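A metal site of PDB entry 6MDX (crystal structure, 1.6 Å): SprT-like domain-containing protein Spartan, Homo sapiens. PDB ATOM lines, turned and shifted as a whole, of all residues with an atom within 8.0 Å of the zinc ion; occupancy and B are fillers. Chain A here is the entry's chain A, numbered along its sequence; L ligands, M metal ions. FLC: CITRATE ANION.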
ATOM      1  N   GLY A  50      13.205 -14.145  19.452  1.00  0.00           N
ATOM      2  CA  GLY A  50      13.187 -14.865  20.703  1.00  0.00           C
ATOM      3  C   GLY A  50      11.975 -15.747  20.784  1.00  0.00           C
ATOM      4  O   GLY A  50      10.902 -15.386  20.238  1.00  0.00           O
ATOM      5  N   ILE A  51      12.117 -16.896  21.432  1.00  0.00           N
ATOM      6  CA  ILE A  51      11.020 -17.788  21.718  1.00  0.00           C
ATOM      7  C   ILE A  51      11.179 -18.369  23.132  1.00  0.00           C
ATOM      8  O   ILE A  51      12.233 -18.393  23.714  1.00  0.00           O
ATOM      9  CB  ILE A  51      10.899 -18.937  20.713  1.00  0.00           C
ATOM     10  CG1 ILE A  51      12.117 -19.875  20.717  1.00  0.00           C
ATOM     11  CG2 ILE A  51      10.668 -18.378  19.324  1.00  0.00           C
ATOM     12  CD1 ILE A  51      11.988 -21.132  21.550  1.00  0.00           C
ATOM     13  N   CYS A  52      10.062 -18.875  23.621  1.00  0.00           N
ATOM     14  CA  CYS A  52      10.017 -19.806  24.709  1.00  0.00           C
ATOM     15  C   CYS A  52       9.431 -21.149  24.285  1.00  0.00           C
ATOM     16  O   CYS A  52       8.651 -21.287  23.380  1.00  0.00           O
ATOM     17  CB  CYS A  52       9.100 -19.300  25.803  1.00  0.00           C
ATOM     18  SG  CYS A  52       9.703 -17.843  26.684  1.00  0.00           S
ATOM     19  N   TYR A  54       7.861 -24.789  26.530  1.00  0.00           N
ATOM     20  CA  TYR A  54       7.425 -25.168  27.854  1.00  0.00           C
ATOM     21  C   TYR A  54       7.367 -26.697  27.923  1.00  0.00           C
ATOM     22  O   TYR A  54       6.841 -27.308  26.999  1.00  0.00           O
ATOM     23  CB  TYR A  54       6.075 -24.508  28.083  1.00  0.00           C
ATOM     24  CG  TYR A  54       6.003 -23.060  27.683  1.00  0.00           C
ATOM     25  CD1 TYR A  54       6.346 -22.068  28.587  1.00  0.00           C
ATOM     26  CD2 TYR A  54       5.577 -22.659  26.413  1.00  0.00           C
ATOM     27  CE1 TYR A  54       6.241 -20.722  28.257  1.00  0.00           C
ATOM     28  CE2 TYR A  54       5.519 -21.311  26.055  1.00  0.00           C
ATOM     29  CZ  TYR A  54       5.855 -20.332  26.991  1.00  0.00           C
ATOM     30  OH  TYR A  54       5.784 -18.990  26.710  1.00  0.00           O
ATOM     31  N   THR A  79      14.601  -8.131  24.145  1.00  0.00           N
ATOM     32  CA  THR A  79      14.022  -9.397  23.708  1.00  0.00           C
ATOM     33  C   THR A  79      14.089 -10.438  24.846  1.00  0.00           C
ATOM     34  O   THR A  79      13.179 -11.193  25.106  1.00  0.00           O
ATOM     35  CB  THR A  79      14.689  -9.971  22.455  1.00  0.00           C
ATOM     36  OG1 THR A  79      14.562  -8.952  21.449  1.00  0.00           O
ATOM     37  CG2 THR A  79      14.112 -11.279  22.011  1.00  0.00           C
ATOM     38  N   HIS A  82      11.570  -9.719  27.505  1.00  0.00           N
ATOM     39  CA  HIS A  82      10.259 -10.067  27.014  1.00  0.00           C
ATOM     40  C   HIS A  82       9.995 -11.561  27.206  1.00  0.00           C
ATOM     41  O   HIS A  82       9.008 -11.988  27.732  1.00  0.00           O
ATOM     42  CB  HIS A  82      10.119  -9.645  25.552  1.00  0.00           C
ATOM     43  CG  HIS A  82       8.819  -9.987  24.910  1.00  0.00           C
ATOM     44  ND1 HIS A  82       7.942  -8.999  24.455  1.00  0.00           N
ATOM     45  CD2 HIS A  82       8.249 -11.168  24.595  1.00  0.00           C
ATOM     46  CE1 HIS A  82       6.884  -9.656  23.907  1.00  0.00           C
ATOM     47  NE2 HIS A  82       7.029 -10.950  23.992  1.00  0.00           N
ATOM     48  N   GLU A  83      10.975 -12.384  26.766  1.00  0.00           N
ATOM     49  CA  GLU A  83      10.823 -13.804  26.884  1.00  0.00           C
ATOM     50  C   GLU A  83      10.824 -14.283  28.364  1.00  0.00           C
ATOM     51  O   GLU A  83      10.076 -15.160  28.710  1.00  0.00           O
ATOM     52  CB  GLU A  83      11.949 -14.550  26.187  1.00  0.00           C
ATOM     53  CG  GLU A  83      12.096 -14.277  24.704  1.00  0.00           C
ATOM     54  CD  GLU A  83      10.832 -14.431  23.877  1.00  0.00           C
ATOM     55  OE1 GLU A  83      10.008 -15.266  24.203  1.00  0.00           O
ATOM     56  OE2 GLU A  83      10.715 -13.669  22.871  1.00  0.00           O
ATOM     57  N   ILE A  85       9.529 -12.621  30.847  1.00  0.00           N
ATOM     58  CA  ILE A  85       8.207 -12.389  31.371  1.00  0.00           C
ATOM     59  C   ILE A  85       7.289 -13.571  31.021  1.00  0.00           C
ATOM     60  O   ILE A  85       6.574 -14.116  31.868  1.00  0.00           O
ATOM     61  CB  ILE A  85       7.616 -11.081  30.887  1.00  0.00           C
ATOM     62  CG1 ILE A  85       8.432  -9.881  31.373  1.00  0.00           C
ATOM     63  CG2 ILE A  85       6.175 -10.994  31.338  1.00  0.00           C
ATOM     64  CD1 ILE A  85       8.023  -8.607  30.676  1.00  0.00           C
ATOM     65  N   HIS A  86       7.342 -14.013  29.744  1.00  0.00           N
ATOM     66  CA  HIS A  86       6.559 -15.237  29.418  1.00  0.00           C
ATOM     67  C   HIS A  86       6.960 -16.411  30.310  1.00  0.00           C
ATOM     68  O   HIS A  86       6.119 -17.179  30.754  1.00  0.00           O
ATOM     69  CB  HIS A  86       6.712 -15.611  27.924  1.00  0.00           C
ATOM     70  CG  HIS A  86       6.066 -14.676  26.939  1.00  0.00           C
ATOM     71  ND1 HIS A  86       4.746 -14.354  26.968  1.00  0.00           N
ATOM     72  CD2 HIS A  86       6.570 -14.082  25.830  1.00  0.00           C
ATOM     73  CE1 HIS A  86       4.476 -13.555  25.926  1.00  0.00           C
ATOM     74  NE2 HIS A  86       5.579 -13.361  25.217  1.00  0.00           N
ATOM     75  N   GLY A 100      -2.000 -13.254  23.955  1.00  0.00           N
ATOM     76  CA  GLY A 100      -0.565 -13.580  24.043  1.00  0.00           C
ATOM     77  C   GLY A 100       0.122 -12.686  25.073  1.00  0.00           C
ATOM     78  O   GLY A 100       0.941 -13.156  25.828  1.00  0.00           O
ATOM     79  N   HIS A 101      -0.230 -11.387  25.062  1.00  0.00           N
ATOM     80  CA  HIS A 101       0.342 -10.361  25.915  1.00  0.00           C
ATOM     81  C   HIS A 101      -0.807  -9.606  26.609  1.00  0.00           C
ATOM     82  O   HIS A 101      -1.109  -8.490  26.194  1.00  0.00           O
ATOM     83  CB  HIS A 101       1.186  -9.388  25.116  1.00  0.00           C
ATOM     84  CG  HIS A 101       2.231 -10.126  24.336  1.00  0.00           C
ATOM     85  ND1 HIS A 101       2.013 -10.499  23.011  1.00  0.00           N
ATOM     86  CD2 HIS A 101       3.445 -10.586  24.695  1.00  0.00           C
ATOM     87  CE1 HIS A 101       3.109 -11.141  22.590  1.00  0.00           C
ATOM     88  NE2 HIS A 101       4.013 -11.228  23.610  1.00  0.00           N
ATOM     89  N   PHE A 105       1.085 -10.071  31.494  1.00  0.00           N
ATOM     90  CA  PHE A 105       2.347  -9.743  30.789  1.00  0.00           C
ATOM     91  C   PHE A 105       2.690  -8.270  30.948  1.00  0.00           C
ATOM     92  O   PHE A 105       3.820  -7.876  31.260  1.00  0.00           O
ATOM     93  CB  PHE A 105       2.237 -10.070  29.292  1.00  0.00           C
ATOM     94  CG  PHE A 105       3.545  -9.917  28.547  1.00  0.00           C
ATOM     95  CD1 PHE A 105       3.956  -8.694  28.061  1.00  0.00           C
ATOM     96  CD2 PHE A 105       4.363 -11.029  28.406  1.00  0.00           C
ATOM     97  CE1 PHE A 105       5.182  -8.548  27.430  1.00  0.00           C
ATOM     98  CE2 PHE A 105       5.608 -10.870  27.799  1.00  0.00           C
ATOM     99  CZ  PHE A 105       5.995  -9.652  27.309  1.00  0.00           C
ATOM    100  N   THR A 121       8.334  -4.219  24.899  1.00  0.00           N
ATOM    101  CA  THR A 121       7.011  -3.976  24.272  1.00  0.00           C
ATOM    102  C   THR A 121       6.317  -5.301  24.015  1.00  0.00           C
ATOM    103  O   THR A 121       6.949  -6.358  24.033  1.00  0.00           O
ATOM    104  CB  THR A 121       7.182  -3.173  22.988  1.00  0.00           C
ATOM    105  OG1 THR A 121       8.092  -3.876  22.123  1.00  0.00           O
ATOM    106  CG2 THR A 121       7.675  -1.771  23.245  1.00  0.00           C
ATOM    107  N   VAL A 122       4.994  -5.242  23.756  1.00  0.00           N
ATOM    108  CA  VAL A 122       4.223  -6.403  23.384  1.00  0.00           C
ATOM    109  C   VAL A 122       4.573  -6.833  21.960  1.00  0.00           C
ATOM    110  O   VAL A 122       4.414  -7.976  21.674  1.00  0.00           O
ATOM    111  CB  VAL A 122       2.704  -6.224  23.541  1.00  0.00           C
ATOM    112  CG1 VAL A 122       2.293  -6.051  25.003  1.00  0.00           C
ATOM    113  CG2 VAL A 122       2.179  -5.066  22.698  1.00  0.00           C
ATOM    114  N   TYR A 123       5.121  -5.916  21.153  1.00  0.00           N
ATOM    115  CA  TYR A 123       5.341  -6.026  19.699  1.00  0.00           C
ATOM    116  C   TYR A 123       6.856  -5.957  19.423  1.00  0.00           C
ATOM    117  O   TYR A 123       7.576  -5.429  20.246  1.00  0.00           O
ATOM    118  CB  TYR A 123       4.554  -4.885  19.028  1.00  0.00           C
ATOM    119  CG  TYR A 123       4.733  -3.494  19.628  1.00  0.00           C
ATOM    120  CD1 TYR A 123       5.846  -2.731  19.327  1.00  0.00           C
ATOM    121  CD2 TYR A 123       3.823  -2.968  20.531  1.00  0.00           C
ATOM    122  CE1 TYR A 123       6.074  -1.494  19.899  1.00  0.00           C
ATOM    123  CE2 TYR A 123       4.002  -1.691  21.090  1.00  0.00           C
ATOM    124  CZ  TYR A 123       5.141  -0.966  20.785  1.00  0.00           C
ATOM    125  OH  TYR A 123       5.359   0.293  21.287  1.00  0.00           O
ATOM    126  N   HIS A 124       7.303  -6.409  18.252  1.00  0.00           N
ATOM    127  CA  HIS A 124       8.727  -6.438  17.834  1.00  0.00           C
ATOM    128  C   HIS A 124       9.114  -5.092  17.213  1.00  0.00           C
ATOM    129  O   HIS A 124       8.320  -4.433  16.559  1.00  0.00           O
ATOM    130  CB  HIS A 124       8.959  -7.657  16.922  1.00  0.00           C
ATOM    131  CG  HIS A 124       8.488  -8.909  17.600  1.00  0.00           C
ATOM    132  ND1 HIS A 124       8.783  -9.162  18.939  1.00  0.00           N
ATOM    133  CD2 HIS A 124       7.723  -9.943  17.187  1.00  0.00           C
ATOM    134  CE1 HIS A 124       8.229 -10.307  19.306  1.00  0.00           C
ATOM    135  NE2 HIS A 124       7.564 -10.805  18.251  1.00  0.00           N
ATOM    136  N   TRP A 137       0.706 -15.880  11.469  1.00  0.00           N
ATOM    137  CA  TRP A 137       1.567 -16.751  12.331  1.00  0.00           C
ATOM    138  C   TRP A 137       0.728 -17.846  12.923  1.00  0.00           C
ATOM    139  O   TRP A 137      -0.385 -17.663  13.390  1.00  0.00           O
ATOM    140  CB  TRP A 137       2.192 -16.021  13.525  1.00  0.00           C
ATOM    141  CG  TRP A 137       3.120 -14.906  13.202  1.00  0.00           C
ATOM    142  CD1 TRP A 137       3.448 -14.323  12.020  1.00  0.00           C
ATOM    143  CD2 TRP A 137       3.950 -14.267  14.191  1.00  0.00           C
ATOM    144  NE1 TRP A 137       4.371 -13.327  12.216  1.00  0.00           N
ATOM    145  CE2 TRP A 137       4.723 -13.301  13.538  1.00  0.00           C
ATOM    146  CE3 TRP A 137       4.121 -14.494  15.563  1.00  0.00           C
ATOM    147  CZ2 TRP A 137       5.655 -12.518  14.209  1.00  0.00           C
ATOM    148  CZ3 TRP A 137       5.030 -13.701  16.229  1.00  0.00           C
ATOM    149  CH2 TRP A 137       5.768 -12.738  15.564  1.00  0.00           C
ATOM    150  N   TYR A 153       6.814 -22.734  15.001  1.00  0.00           N
ATOM    151  CA  TYR A 153       6.204 -21.560  14.268  1.00  0.00           C
ATOM    152  C   TYR A 153       6.158 -21.780  12.770  1.00  0.00           C
ATOM    153  O   TYR A 153       7.049 -22.382  12.191  1.00  0.00           O
ATOM    154  CB  TYR A 153       6.988 -20.273  14.566  1.00  0.00           C
ATOM    155  CG  TYR A 153       6.798 -19.746  15.949  1.00  0.00           C
ATOM    156  CD1 TYR A 153       5.731 -18.922  16.254  1.00  0.00           C
ATOM    157  CD2 TYR A 153       7.661 -20.070  16.993  1.00  0.00           C
ATOM    158  CE1 TYR A 153       5.506 -18.455  17.543  1.00  0.00           C
ATOM    159  CE2 TYR A 153       7.414 -19.644  18.283  1.00  0.00           C
ATOM    160  CZ  TYR A 153       6.360 -18.814  18.560  1.00  0.00           C
ATOM    161  OH  TYR A 153       6.130 -18.333  19.832  1.00  0.00           O
HETATM  162  CAC FLC L   1       7.345 -14.822  22.353  1.00  0.00           C
HETATM  163  CA  FLC L   1       6.351 -15.189  21.265  1.00  0.00           C
HETATM  164  CB  FLC L   1       5.196 -14.194  21.117  1.00  0.00           C
HETATM  165  CBC FLC L   1       5.851 -12.903  20.602  1.00  0.00           C
HETATM  166  CG  FLC L   1       4.242 -14.792  20.087  1.00  0.00           C
HETATM  167  CGC FLC L   1       2.896 -14.090  20.096  1.00  0.00           C
HETATM  168  OA1 FLC L   1       8.192 -15.708  22.619  1.00  0.00           O
HETATM  169  OA2 FLC L   1       7.282 -13.656  22.884  1.00  0.00           O
HETATM  170  OB1 FLC L   1       6.338 -13.004  19.447  1.00  0.00           O
HETATM  171  OB2 FLC L   1       5.871 -11.887  21.388  1.00  0.00           O
HETATM  172  OG1 FLC L   1       1.897 -14.750  20.495  1.00  0.00           O
HETATM  173  OG2 FLC L   1       2.906 -12.870  19.758  1.00  0.00           O
HETATM  174  OHB FLC L   1       4.569 -13.915  22.383  1.00  0.00           O
HETATM  175 ZN    ZN M   1       5.698 -12.376  23.406  1.00  0.00          ZN
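The zinc ion is bound by NE2 of His 82. The zinc ion is bound by NE2 of His 101. The zinc ion is bound by a ring nitrogen (NE2) of His 86 (2.1 Å). An oxygen (OB2) of the ligand is bound to the zinc ion, 2.1 Å away. OA2 of the ligand binds the zinc ion (2.1 Å). The zinc ion is bound by an oxygen (OHB) of the ligand, 2.2 Å away.
A ring nitrogen (ND1) of His 82 is in hydrogen-bond range of the backbone carbonyl oxygen (O) of Thr 121, 2.9 Å away.
The nearest printed residue that does not touch the zinc ion is Phe 105 (4.6 Å).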
